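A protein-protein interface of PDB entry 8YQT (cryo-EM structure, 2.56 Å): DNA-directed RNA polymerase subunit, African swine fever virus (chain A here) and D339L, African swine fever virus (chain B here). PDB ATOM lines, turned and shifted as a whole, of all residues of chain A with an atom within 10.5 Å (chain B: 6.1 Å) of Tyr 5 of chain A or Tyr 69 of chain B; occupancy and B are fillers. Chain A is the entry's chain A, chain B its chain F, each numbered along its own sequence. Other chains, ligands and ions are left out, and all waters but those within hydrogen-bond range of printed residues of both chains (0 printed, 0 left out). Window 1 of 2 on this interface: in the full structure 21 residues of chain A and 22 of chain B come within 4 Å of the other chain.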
ATOM      1  N   GLU A   2     -10.387  35.413  21.450  1.00  0.00           N
ATOM      2  CA  GLU A   2     -11.593  34.896  20.826  1.00  0.00           C
ATOM      3  C   GLU A   2     -12.816  35.323  21.626  1.00  0.00           C
ATOM      4  O   GLU A   2     -12.751  35.505  22.845  1.00  0.00           O
ATOM      5  CB  GLU A   2     -11.554  33.368  20.704  1.00  0.00           C
ATOM      6  CG  GLU A   2     -11.908  32.620  21.979  1.00  0.00           C
ATOM      7  CD  GLU A   2     -12.219  31.158  21.730  1.00  0.00           C
ATOM      8  OE1 GLU A   2     -12.111  30.713  20.569  1.00  0.00           O
ATOM      9  OE2 GLU A   2     -12.580  30.454  22.695  1.00  0.00           O
ATOM     10  N   ALA A   3     -13.928  35.499  20.920  1.00  0.00           N
ATOM     11  CA  ALA A   3     -15.204  35.830  21.541  1.00  0.00           C
ATOM     12  C   ALA A   3     -15.920  34.530  21.880  1.00  0.00           C
ATOM     13  O   ALA A   3     -16.279  33.760  20.983  1.00  0.00           O
ATOM     14  CB  ALA A   3     -16.046  36.701  20.615  1.00  0.00           C
ATOM     15  N   GLY A   4     -16.116  34.278  23.167  1.00  0.00           N
ATOM     16  CA  GLY A   4     -16.758  33.057  23.597  1.00  0.00           C
ATOM     17  C   GLY A   4     -18.242  33.043  23.293  1.00  0.00           C
ATOM     18  O   GLY A   4     -18.876  34.065  23.042  1.00  0.00           O
ATOM     19  N   TYR A   5     -18.802  31.839  23.313  1.00  0.00           N
ATOM     20  CA  TYR A   5     -20.222  31.663  23.049  1.00  0.00           C
ATOM     21  C   TYR A   5     -21.053  32.316  24.144  1.00  0.00           C
ATOM     22  O   TYR A   5     -20.749  32.196  25.333  1.00  0.00           O
ATOM     23  CB  TYR A   5     -20.556  30.175  22.950  1.00  0.00           C
ATOM     24  CG  TYR A   5     -21.999  29.883  22.633  1.00  0.00           C
ATOM     25  CD1 TYR A   5     -22.477  29.974  21.335  1.00  0.00           C
ATOM     26  CD2 TYR A   5     -22.885  29.515  23.631  1.00  0.00           C
ATOM     27  CE1 TYR A   5     -23.795  29.706  21.046  1.00  0.00           C
ATOM     28  CE2 TYR A   5     -24.198  29.244  23.349  1.00  0.00           C
ATOM     29  CZ  TYR A   5     -24.648  29.341  22.060  1.00  0.00           C
ATOM     30  OH  TYR A   5     -25.963  29.071  21.782  1.00  0.00           O
ATOM     31  N   ALA A   6     -22.115  33.007  23.740  1.00  0.00           N
ATOM     32  CA  ALA A   6     -22.982  33.679  24.693  1.00  0.00           C
ATOM     33  C   ALA A   6     -24.401  33.709  24.151  1.00  0.00           C
ATOM     34  O   ALA A   6     -24.632  33.575  22.948  1.00  0.00           O
ATOM     35  CB  ALA A   6     -22.493  35.098  24.997  1.00  0.00           C
ATOM     36  N   GLU A   7     -25.351  33.876  25.066  1.00  0.00           N
ATOM     37  CA  GLU A   7     -26.756  34.048  24.732  1.00  0.00           C
ATOM     38  C   GLU A   7     -27.302  35.240  25.497  1.00  0.00           C
ATOM     39  O   GLU A   7     -26.873  35.524  26.616  1.00  0.00           O
ATOM     40  CB  GLU A   7     -27.584  32.801  25.066  1.00  0.00           C
ATOM     41  CG  GLU A   7     -26.887  31.490  24.783  1.00  0.00           C
ATOM     42  CD  GLU A   7     -27.852  30.382  24.427  1.00  0.00           C
ATOM     43  OE1 GLU A   7     -29.073  30.641  24.398  1.00  0.00           O
ATOM     44  OE2 GLU A   7     -27.390  29.250  24.179  1.00  0.00           O
ATOM     45  N   ILE A   8     -28.256  35.935  24.889  1.00  0.00           N
ATOM     46  CA  ILE A   8     -28.887  37.082  25.532  1.00  0.00           C
ATOM     47  C   ILE A   8     -29.942  36.579  26.508  1.00  0.00           C
ATOM     48  O   ILE A   8     -30.890  35.892  26.114  1.00  0.00           O
ATOM     49  CB  ILE A   8     -29.497  38.030  24.492  1.00  0.00           C
ATOM     50  CG1 ILE A   8     -28.393  38.643  23.632  1.00  0.00           C
ATOM     51  CG2 ILE A   8     -30.307  39.114  25.170  1.00  0.00           C
ATOM     52  CD1 ILE A   8     -28.896  39.320  22.388  1.00  0.00           C
ATOM     53  N   ALA A   9     -29.782  36.921  27.785  1.00  0.00           N
ATOM     54  CA  ALA A   9     -30.725  36.500  28.813  1.00  0.00           C
ATOM     55  C   ALA A   9     -31.818  37.525  29.068  1.00  0.00           C
ATOM     56  O   ALA A   9     -32.936  37.148  29.431  1.00  0.00           O
ATOM     57  CB  ALA A   9     -29.992  36.213  30.125  1.00  0.00           C
ATOM     58  N   GLY A1417     -33.269  37.901  17.250  1.00  0.00           N
ATOM     59  CA  GLY A1417     -32.472  37.136  16.316  1.00  0.00           C
ATOM     60  C   GLY A1417     -32.066  35.764  16.792  1.00  0.00           C
ATOM     61  O   GLY A1417     -31.259  35.110  16.125  1.00  0.00           O
ATOM     62  N   SER A1418     -32.595  35.306  17.916  1.00  0.00           N
ATOM     63  CA  SER A1418     -32.237  34.030  18.503  1.00  0.00           C
ATOM     64  C   SER A1418     -33.321  32.995  18.207  1.00  0.00           C
ATOM     65  O   SER A1418     -34.250  33.233  17.432  1.00  0.00           O
ATOM     66  CB  SER A1418     -32.003  34.201  20.002  1.00  0.00           C
ATOM     67  OG  SER A1418     -31.679  32.966  20.611  1.00  0.00           O
ATOM     68  N   VAL A1419     -33.199  31.826  18.827  1.00  0.00           N
ATOM     69  CA  VAL A1419     -34.149  30.736  18.635  1.00  0.00           C
ATOM     70  C   VAL A1419     -34.786  30.413  19.983  1.00  0.00           C
ATOM     71  O   VAL A1419     -34.091  30.399  21.008  1.00  0.00           O
ATOM     72  CB  VAL A1419     -33.459  29.512  18.004  1.00  0.00           C
ATOM     73  CG1 VAL A1419     -32.294  29.041  18.858  1.00  0.00           C
ATOM     74  CG2 VAL A1419     -34.447  28.387  17.761  1.00  0.00           C
ATOM     75  N   PRO A1420     -36.098  30.190  20.040  1.00  0.00           N
ATOM     76  CA  PRO A1420     -36.740  29.881  21.324  1.00  0.00           C
ATOM     77  C   PRO A1420     -36.192  28.614  21.961  1.00  0.00           C
ATOM     78  O   PRO A1420     -35.879  27.636  21.280  1.00  0.00           O
ATOM     79  CB  PRO A1420     -38.215  29.717  20.947  1.00  0.00           C
ATOM     80  CG  PRO A1420     -38.374  30.530  19.727  1.00  0.00           C
ATOM     81  CD  PRO A1420     -37.087  30.421  18.975  1.00  0.00           C
ATOM     82  N   ARG A1421     -36.085  28.640  23.288  1.00  0.00           N
ATOM     83  CA  ARG A1421     -35.689  27.466  24.066  1.00  0.00           C
ATOM     84  C   ARG A1421     -36.929  26.600  24.293  1.00  0.00           C
ATOM     85  O   ARG A1421     -37.601  26.649  25.322  1.00  0.00           O
ATOM     86  CB  ARG A1421     -35.024  27.892  25.369  1.00  0.00           C
ATOM     87  CG  ARG A1421     -34.803  26.781  26.381  1.00  0.00           C
ATOM     88  CD  ARG A1421     -33.446  26.886  27.049  1.00  0.00           C
ATOM     89  NE  ARG A1421     -32.964  28.260  27.113  1.00  0.00           N
ATOM     90  CZ  ARG A1421     -31.684  28.603  27.112  1.00  0.00           C
ATOM     91  NH1 ARG A1421     -30.725  27.694  27.045  1.00  0.00           N
ATOM     92  NH2 ARG A1421     -31.356  29.889  27.176  1.00  0.00           N
ATOM     93  N   MET A1425     -34.726  22.244  21.973  1.00  0.00           N
ATOM     94  CA  MET A1425     -33.793  23.128  22.651  1.00  0.00           C
ATOM     95  C   MET A1425     -34.187  23.403  24.090  1.00  0.00           C
ATOM     96  O   MET A1425     -33.601  24.284  24.722  1.00  0.00           O
ATOM     97  CB  MET A1425     -33.665  24.441  21.885  1.00  0.00           C
ATOM     98  CG  MET A1425     -33.433  24.218  20.420  1.00  0.00           C
ATOM     99  SD  MET A1425     -31.769  23.673  20.040  1.00  0.00           S
ATOM    100  CE  MET A1425     -31.573  24.431  18.444  1.00  0.00           C
ATOM    101  N   SER A1427     -33.880  21.235  26.669  1.00  0.00           N
ATOM    102  CA  SER A1427     -32.878  20.631  27.531  1.00  0.00           C
ATOM    103  C   SER A1427     -31.484  20.874  26.969  1.00  0.00           C
ATOM    104  O   SER A1427     -31.286  20.929  25.753  1.00  0.00           O
ATOM    105  CB  SER A1427     -33.117  19.129  27.684  1.00  0.00           C
ATOM    106  OG  SER A1427     -34.359  18.873  28.309  1.00  0.00           O
ATOM    107  N   ASP A1428     -30.520  21.021  27.870  1.00  0.00           N
ATOM    108  CA  ASP A1428     -29.133  21.224  27.486  1.00  0.00           C
ATOM    109  C   ASP A1428     -28.415  19.889  27.372  1.00  0.00           C
ATOM    110  O   ASP A1428     -28.635  18.978  28.174  1.00  0.00           O
ATOM    111  CB  ASP A1428     -28.412  22.113  28.498  1.00  0.00           C
ATOM    112  CG  ASP A1428     -29.121  23.429  28.723  1.00  0.00           C
ATOM    113  OD1 ASP A1428     -29.829  23.895  27.805  1.00  0.00           O
ATOM    114  OD2 ASP A1428     -28.965  24.004  29.820  1.00  0.00           O
ATOM    115  N   ILE A1429     -27.560  19.776  26.364  1.00  0.00           N
ATOM    116  CA  ILE A1429     -26.724  18.601  26.168  1.00  0.00           C
ATOM    117  C   ILE A1429     -25.301  18.963  26.565  1.00  0.00           C
ATOM    118  O   ILE A1429     -24.771  19.991  26.129  1.00  0.00           O
ATOM    119  CB  ILE A1429     -26.781  18.107  24.713  1.00  0.00           C
ATOM    120  CG1 ILE A1429     -28.230  17.997  24.237  1.00  0.00           C
ATOM    121  CG2 ILE A1429     -26.086  16.770  24.587  1.00  0.00           C
ATOM    122  CD1 ILE A1429     -29.057  17.016  25.017  1.00  0.00           C
ATOM    123  N   ILE A1430     -24.689  18.133  27.403  1.00  0.00           N
ATOM    124  CA  ILE A1430     -23.300  18.316  27.790  1.00  0.00           C
ATOM    125  C   ILE A1430     -22.530  17.058  27.421  1.00  0.00           C
ATOM    126  O   ILE A1430     -23.088  15.965  27.309  1.00  0.00           O
ATOM    127  CB  ILE A1430     -23.139  18.640  29.290  1.00  0.00           C
ATOM    128  CG1 ILE A1430     -23.538  17.445  30.148  1.00  0.00           C
ATOM    129  CG2 ILE A1430     -23.960  19.850  29.662  1.00  0.00           C
ATOM    130  CD1 ILE A1430     -23.341  17.668  31.622  1.00  0.00           C
ATOM    131  N   MET A1431     -21.231  17.230  27.215  1.00  0.00           N
ATOM    132  CA  MET A1431     -20.373  16.116  26.850  1.00  0.00           C
ATOM    133  C   MET A1431     -20.156  15.221  28.062  1.00  0.00           C
ATOM    134  O   MET A1431     -20.003  15.704  29.187  1.00  0.00           O
ATOM    135  CB  MET A1431     -19.034  16.632  26.333  1.00  0.00           C
ATOM    136  CG  MET A1431     -19.072  17.207  24.924  1.00  0.00           C
ATOM    137  SD  MET A1431     -19.987  16.240  23.721  1.00  0.00           S
ATOM    138  CE  MET A1431     -18.751  15.062  23.211  1.00  0.00           C
ATOM    139  N   GLU A1433     -17.775  13.476  29.895  1.00  0.00           N
ATOM    140  CA  GLU A1433     -16.325  13.389  30.022  1.00  0.00           C
ATOM    141  C   GLU A1433     -15.892  12.060  30.628  1.00  0.00           C
ATOM    142  O   GLU A1433     -14.950  11.429  30.137  1.00  0.00           O
ATOM    143  CB  GLU A1433     -15.807  14.548  30.868  1.00  0.00           C
ATOM    144  CG  GLU A1433     -16.286  15.908  30.413  1.00  0.00           C
ATOM    145  CD  GLU A1433     -15.874  17.006  31.364  1.00  0.00           C
ATOM    146  OE1 GLU A1433     -15.005  16.749  32.222  1.00  0.00           O
ATOM    147  OE2 GLU A1433     -16.422  18.123  31.259  1.00  0.00           O
ATOM    148  N   THR B  10     -14.987  32.360  28.425  1.00  0.00           N
ATOM    149  CA  THR B  10     -15.703  31.277  27.766  1.00  0.00           C
ATOM    150  C   THR B  10     -14.895  30.844  26.554  1.00  0.00           C
ATOM    151  O   THR B  10     -14.569  31.671  25.695  1.00  0.00           O
ATOM    152  CB  THR B  10     -17.114  31.703  27.352  1.00  0.00           C
ATOM    153  OG1 THR B  10     -17.898  31.976  28.517  1.00  0.00           O
ATOM    154  CG2 THR B  10     -17.789  30.606  26.551  1.00  0.00           C
ATOM    155  N   LEU B  11     -14.571  29.560  26.487  1.00  0.00           N
ATOM    156  CA  LEU B  11     -13.826  28.995  25.373  1.00  0.00           C
ATOM    157  C   LEU B  11     -14.762  28.226  24.454  1.00  0.00           C
ATOM    158  O   LEU B  11     -15.625  27.474  24.918  1.00  0.00           O
ATOM    159  CB  LEU B  11     -12.715  28.067  25.867  1.00  0.00           C
ATOM    160  CG  LEU B  11     -11.612  28.695  26.714  1.00  0.00           C
ATOM    161  CD1 LEU B  11     -10.524  27.680  27.001  1.00  0.00           C
ATOM    162  CD2 LEU B  11     -11.040  29.915  26.027  1.00  0.00           C
ATOM    163  N   ASN B  12     -14.590  28.429  23.152  1.00  0.00           N
ATOM    164  CA  ASN B  12     -15.277  27.635  22.146  1.00  0.00           C
ATOM    165  C   ASN B  12     -14.471  26.376  21.866  1.00  0.00           C
ATOM    166  O   ASN B  12     -13.239  26.387  21.926  1.00  0.00           O
ATOM    167  CB  ASN B  12     -15.465  28.432  20.856  1.00  0.00           C
ATOM    168  CG  ASN B  12     -16.283  29.683  21.062  1.00  0.00           C
ATOM    169  OD1 ASN B  12     -17.231  29.697  21.842  1.00  0.00           O
ATOM    170  ND2 ASN B  12     -15.925  30.744  20.354  1.00  0.00           N
ATOM    171  N   ILE B  13     -15.171  25.290  21.556  1.00  0.00           N
ATOM    172  CA  ILE B  13     -14.566  23.974  21.399  1.00  0.00           C
ATOM    173  C   ILE B  13     -15.106  23.394  20.100  1.00  0.00           C
ATOM    174  O   ILE B  13     -16.269  22.986  20.031  1.00  0.00           O
ATOM    175  CB  ILE B  13     -14.869  23.055  22.584  1.00  0.00           C
ATOM    176  CG1 ILE B  13     -14.296  23.649  23.871  1.00  0.00           C
ATOM    177  CG2 ILE B  13     -14.306  21.682  22.336  1.00  0.00           C
ATOM    178  CD1 ILE B  13     -14.839  23.030  25.121  1.00  0.00           C
ATOM    179  N   SER B  55     -16.801  24.773  33.933  1.00  0.00           N
ATOM    180  CA  SER B  55     -18.121  24.224  33.675  1.00  0.00           C
ATOM    181  C   SER B  55     -18.013  22.958  32.843  1.00  0.00           C
ATOM    182  O   SER B  55     -16.953  22.643  32.296  1.00  0.00           O
ATOM    183  CB  SER B  55     -18.982  25.257  32.950  1.00  0.00           C
ATOM    184  OG  SER B  55     -18.684  25.292  31.567  1.00  0.00           O
ATOM    185  N   PRO B  56     -19.094  22.192  32.732  1.00  0.00           N
ATOM    186  CA  PRO B  56     -19.130  21.118  31.738  1.00  0.00           C
ATOM    187  C   PRO B  56     -19.053  21.680  30.328  1.00  0.00           C
ATOM    188  O   PRO B  56     -19.245  22.873  30.090  1.00  0.00           O
ATOM    189  CB  PRO B  56     -20.481  20.441  31.990  1.00  0.00           C
ATOM    190  CG  PRO B  56     -20.815  20.779  33.385  1.00  0.00           C
ATOM    191  CD  PRO B  56     -20.267  22.147  33.622  1.00  0.00           C
ATOM    192  N   CYS B  57     -18.761  20.797  29.381  1.00  0.00           N
ATOM    193  CA  CYS B  57     -18.712  21.191  27.977  1.00  0.00           C
ATOM    194  C   CYS B  57     -20.135  21.213  27.436  1.00  0.00           C
ATOM    195  O   CYS B  57     -20.673  20.183  27.027  1.00  0.00           O
ATOM    196  CB  CYS B  57     -17.827  20.243  27.178  1.00  0.00           C
ATOM    197  SG  CYS B  57     -17.663  20.683  25.435  1.00  0.00           S
ATOM    198  N   PHE B  58     -20.752  22.389  27.440  1.00  0.00           N
ATOM    199  CA  PHE B  58     -22.075  22.544  26.860  1.00  0.00           C
ATOM    200  C   PHE B  58     -21.989  22.523  25.341  1.00  0.00           C
ATOM    201  O   PHE B  58     -20.999  22.952  24.751  1.00  0.00           O
ATOM    202  CB  PHE B  58     -22.718  23.857  27.302  1.00  0.00           C
ATOM    203  CG  PHE B  58     -22.758  24.054  28.781  1.00  0.00           C
ATOM    204  CD1 PHE B  58     -23.656  23.356  29.561  1.00  0.00           C
ATOM    205  CD2 PHE B  58     -21.919  24.965  29.392  1.00  0.00           C
ATOM    206  CE1 PHE B  58     -23.701  23.546  30.920  1.00  0.00           C
ATOM    207  CE2 PHE B  58     -21.963  25.159  30.751  1.00  0.00           C
ATOM    208  CZ  PHE B  58     -22.855  24.449  31.516  1.00  0.00           C
ATOM    209  N   ILE B  59     -23.039  22.030  24.712  1.00  0.00           N
ATOM    210  CA  ILE B  59     -23.157  22.067  23.259  1.00  0.00           C
ATOM    211  C   ILE B  59     -23.890  23.340  22.868  1.00  0.00           C
ATOM    212  O   ILE B  59     -24.894  23.707  23.485  1.00  0.00           O
ATOM    213  CB  ILE B  59     -23.879  20.814  22.731  1.00  0.00           C
ATOM    214  CG1 ILE B  59     -23.163  19.551  23.208  1.00  0.00           C
ATOM    215  CG2 ILE B  59     -23.949  20.838  21.220  1.00  0.00           C
ATOM    216  CD1 ILE B  59     -21.727  19.464  22.770  1.00  0.00           C
ATOM    217  N   MET B  60     -23.375  24.028  21.851  1.00  0.00           N
ATOM    218  CA  MET B  60     -23.976  25.279  21.411  1.00  0.00           C
ATOM    219  C   MET B  60     -25.415  25.061  20.971  1.00  0.00           C
ATOM    220  O   MET B  60     -25.731  24.094  20.273  1.00  0.00           O
ATOM    221  CB  MET B  60     -23.162  25.889  20.275  1.00  0.00           C
ATOM    222  CG  MET B  60     -21.857  26.506  20.725  1.00  0.00           C
ATOM    223  SD  MET B  60     -20.994  27.362  19.403  1.00  0.00           S
ATOM    224  CE  MET B  60     -19.306  27.206  19.967  1.00  0.00           C
ATOM    225  N   ARG B  61     -26.289  25.978  21.376  1.00  0.00           N
ATOM    226  CA  ARG B  61     -27.726  25.789  21.260  1.00  0.00           C
ATOM    227  C   ARG B  61     -28.371  26.626  20.166  1.00  0.00           C
ATOM    228  O   ARG B  61     -29.484  26.305  19.748  1.00  0.00           O
ATOM    229  CB  ARG B  61     -28.398  26.117  22.597  1.00  0.00           C
ATOM    230  CG  ARG B  61     -29.693  25.388  22.858  1.00  0.00           C
ATOM    231  CD  ARG B  61     -30.633  26.247  23.682  1.00  0.00           C
ATOM    232  NE  ARG B  61     -31.434  27.135  22.848  1.00  0.00           N
ATOM    233  CZ  ARG B  61     -31.570  28.438  23.052  1.00  0.00           C
ATOM    234  NH1 ARG B  61     -30.964  29.048  24.055  1.00  0.00           N
ATOM    235  NH2 ARG B  61     -32.331  29.147  22.224  1.00  0.00           N
ATOM    236  N   THR B  62     -27.719  27.684  19.695  1.00  0.00           N
ATOM    237  CA  THR B  62     -28.334  28.600  18.744  1.00  0.00           C
ATOM    238  C   THR B  62     -27.855  28.385  17.316  1.00  0.00           C
ATOM    239  O   THR B  62     -28.128  29.220  16.450  1.00  0.00           O
ATOM    240  CB  THR B  62     -28.085  30.048  19.167  1.00  0.00           C
ATOM    241  OG1 THR B  62     -26.684  30.249  19.377  1.00  0.00           O
ATOM    242  CG2 THR B  62     -28.831  30.357  20.448  1.00  0.00           C
ATOM    243  N   ASN B  63     -27.144  27.295  17.048  1.00  0.00           N
ATOM    244  CA  ASN B  63     -26.713  26.982  15.696  1.00  0.00           C
ATOM    245  C   ASN B  63     -26.596  25.473  15.563  1.00  0.00           C
ATOM    246  O   ASN B  63     -26.652  24.735  16.548  1.00  0.00           O
ATOM    247  CB  ASN B  63     -25.395  27.682  15.342  1.00  0.00           C
ATOM    248  CG  ASN B  63     -24.309  27.448  16.369  1.00  0.00           C
ATOM    249  OD1 ASN B  63     -24.495  26.712  17.333  1.00  0.00           O
ATOM    250  ND2 ASN B  63     -23.167  28.084  16.170  1.00  0.00           N
ATOM    251  N   ARG B  67     -20.858  22.318  17.926  1.00  0.00           N
ATOM    252  CA  ARG B  67     -19.687  22.768  18.654  1.00  0.00           C
ATOM    253  C   ARG B  67     -20.027  22.980  20.122  1.00  0.00           C
ATOM    254  O   ARG B  67     -21.177  23.222  20.490  1.00  0.00           O
ATOM    255  CB  ARG B  67     -19.150  24.059  18.037  1.00  0.00           C
ATOM    256  CG  ARG B  67     -18.127  23.831  16.951  1.00  0.00           C
ATOM    257  CD  ARG B  67     -18.079  24.985  15.973  1.00  0.00           C
ATOM    258  NE  ARG B  67     -17.454  26.173  16.541  1.00  0.00           N
ATOM    259  CZ  ARG B  67     -18.034  27.362  16.608  1.00  0.00           C
ATOM    260  NH1 ARG B  67     -19.258  27.561  16.148  1.00  0.00           N
ATOM    261  NH2 ARG B  67     -17.368  28.379  17.147  1.00  0.00           N
ATOM    262  N   GLY B  68     -19.002  22.874  20.964  1.00  0.00           N
ATOM    263  CA  GLY B  68     -19.151  23.023  22.391  1.00  0.00           C
ATOM    264  C   GLY B  68     -18.607  24.349  22.895  1.00  0.00           C
ATOM    265  O   GLY B  68     -17.970  25.112  22.177  1.00  0.00           O
ATOM    266  N   TYR B  69     -18.869  24.610  24.170  1.00  0.00           N
ATOM    267  CA  TYR B  69     -18.296  25.774  24.826  1.00  0.00           C
ATOM    268  C   TYR B  69     -18.185  25.481  26.312  1.00  0.00           C
ATOM    269  O   TYR B  69     -18.898  24.634  26.851  1.00  0.00           O
ATOM    270  CB  TYR B  69     -19.121  27.038  24.562  1.00  0.00           C
ATOM    271  CG  TYR B  69     -20.479  27.059  25.219  1.00  0.00           C
ATOM    272  CD1 TYR B  69     -21.578  26.489  24.599  1.00  0.00           C
ATOM    273  CD2 TYR B  69     -20.665  27.668  26.449  1.00  0.00           C
ATOM    274  CE1 TYR B  69     -22.819  26.515  25.189  1.00  0.00           C
ATOM    275  CE2 TYR B  69     -21.898  27.696  27.046  1.00  0.00           C
ATOM    276  CZ  TYR B  69     -22.974  27.120  26.414  1.00  0.00           C
ATOM    277  OH  TYR B  69     -24.210  27.149  27.013  1.00  0.00           O
ATOM    278  N   MET B  70     -17.274  26.194  26.965  1.00  0.00           N
ATOM    279  CA  MET B  70     -16.967  25.926  28.362  1.00  0.00           C
ATOM    280  C   MET B  70     -16.625  27.228  29.067  1.00  0.00           C
ATOM    281  O   MET B  70     -15.903  28.060  28.522  1.00  0.00           O
ATOM    282  CB  MET B  70     -15.804  24.935  28.487  1.00  0.00           C
ATOM    283  CG  MET B  70     -15.481  24.521  29.909  1.00  0.00           C
ATOM    284  SD  MET B  70     -14.080  23.396  30.000  1.00  0.00           S
ATOM    285  CE  MET B  70     -14.810  21.891  29.373  1.00  0.00           C
ATOM    286  N   HIS B  71     -17.137  27.394  30.280  1.00  0.00           N
ATOM    287  CA  HIS B  71     -16.801  28.539  31.116  1.00  0.00           C
ATOM    288  C   HIS B  71     -15.620  28.171  32.002  1.00  0.00           C
ATOM    289  O   HIS B  71     -15.676  27.180  32.734  1.00  0.00           O
ATOM    290  CB  HIS B  71     -17.991  28.967  31.975  1.00  0.00           C
ATOM    291  CG  HIS B  71     -19.238  29.236  31.194  1.00  0.00           C
ATOM    292  ND1 HIS B  71     -19.275  30.104  30.124  1.00  0.00           N
ATOM    293  CD2 HIS B  71     -20.500  28.768  31.340  1.00  0.00           C
ATOM    294  CE1 HIS B  71     -20.502  30.149  29.639  1.00  0.00           C
ATOM    295  NE2 HIS B  71     -21.265  29.348  30.359  1.00  0.00           N
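The side-chain carboxylate (OE2) of Glu 2 of chain A lies within hydrogen-bond range of the backbone NH (N) of Asn 12 of chain B (2.9 Å).
O of Ala 3 of chain A sits at hydrogen-bond distance from ND2 of Asn 12 of chain B (3.1 Å).
The backbone NH (N) of Tyr 5 of chain A lies within hydrogen-bond range of the side-chain amide oxygen (OD1) of Asn 12 of chain B, at 3.0 Å.
N of Arg 61 of chain B lies within hydrogen-bond range of OH of Tyr 5 of chain A, 3.1 Å away.
The side-chain hydroxyl (OG1) of Thr 62 of chain B sits at hydrogen-bond distance from the side-chain hydroxyl (OH) of Tyr 5 of chain A, 2.8 Å away.
OE1 of Glu 7 of chain A is in salt-bridge range of NH1 of Arg 61 of chain B, 2.5 Å away.
The backbone carbonyl oxygen (O) of Val 1419 of chain A is in hydrogen-bond range of the guanidinium group (NH2) of Arg 61 of chain B, at 2.5 Å.
The backbone carbonyl oxygen of Ile 1429 of chain A sits at hydrogen-bond distance from the backbone NH of Ile 59 of chain B, at 3.0 Å.
The backbone NH (N) of Met 1431 of chain A is in hydrogen-bond range of the backbone carbonyl oxygen (O) of Cys 57 of chain B (3.0 Å).
NH1 of Arg 61 of chain B lies close to NH2 of Arg 1421 of chain A, 3.3 Å away.
O of Arg 61 of chain B sits close to SD of Met 1425 of chain A, at 3.5 Å.
The guanidinium group (NH2) of Arg 1421 of chain A is in salt-bridge range of the side-chain carboxylate (OE1) of Glu 7 of chain A, at 3.7 Å.
O of Met 70 of chain B lies within hydrogen-bond range of N of Leu 11 of chain B (2.9 Å).
The backbone NH (N) of Tyr 69 of chain B is in hydrogen-bond range of the backbone carbonyl oxygen (O) of Phe 58 of chain B, at 2.8 Å.
Among the printed residues, pairs that only touch across the chains: Glu 2 of chain A with Thr 10 of chain B (3.8 Å), Glu 2 of chain A with Leu 11 of chain B (3.3 Å), Gly 4 of chain A with Thr 10 of chain B (3.3 Å), Gly 4 of chain A with Asn 12 of chain B (3.8 Å), Tyr 5 of chain A with Thr 10 of chain B (3.6 Å), Tyr 5 of chain A with Met 60 of chain B (3.6 Å), Tyr 5 of chain A with Tyr 69 of chain B (3.4 Å), Glu 7 of chain A with Thr 62 of chain B (3.97 Å), Ser 1418 of chain A with Thr 62 of chain B (3.9 Å), Val 1419 of chain A with Thr 62 of chain B (3.99 Å), Pro 1420 of chain A with Arg 61 of chain B (3.9 Å), Ile 1429 of chain A with Phe 58 of chain B (3.8 Å), Ile 1430 of chain A with Cys 57 of chain B (3.3 Å), Ile 1430 of chain A with Phe 58 of chain B (3.5 Å) and Met 1431 of chain A with Ile 59 of chain B (3.8 Å).
Printed residues of chain B within 4 Å of Glu 7 of chain A: Arg 61 and Thr 62.
Ala 9 of chain A touches none of the printed residues of chain B.
Asp 1428 of chain A touches none of the printed residues of chain B.
Of the printed residues of chain A, Thr 10 of chain B touches Glu 2, Gly 4 and Tyr 5.
No residue of chain A comes within 4 Å of Ile 13 of chain B.
No residue of chain A comes within 4 Å of Gly 68 of chain B.
Of chain A, only Tyr 5 comes within 4 Å of Tyr 69 of chain B.
Met 70 of chain B touches none of the printed residues of chain A.
The nearest residue of chain A that does not touch Tyr 69 of chain B is Glu 7 of chain A (4.7 Å).
The nearest printed residue of chain B that does not touch Ser 1418 of chain A is Arg 61 of chain B (4.2 Å).
Printed residues of chain B that touch a printed residue of chain A: Thr 10, Leu 11, Asn 12, Cys 57, Phe 58, Ile 59, Met 60, Arg 61, Thr 62 and Tyr 69.
Hydrophobic or aromatic side chains of chain B that line the printed part of chain A: Leu 11, Phe 58, Ile 59, Met 60 and Tyr 69.
Of the 20 printed residues of chain A, 13 touch a printed residue of chain B.
Hydrophobic or aromatic side chains of chain A within 4 Å of the printed part of chain B: Tyr 5, Val 1419, Met 1425, Ile 1430 and Met 1431.
Among the printed residues, Asp or Glu carboxylates within 4 Å of a Lys or Arg side-chain nitrogen of the other chain: Glu 7 of chain A with Arg 61 of chain B.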
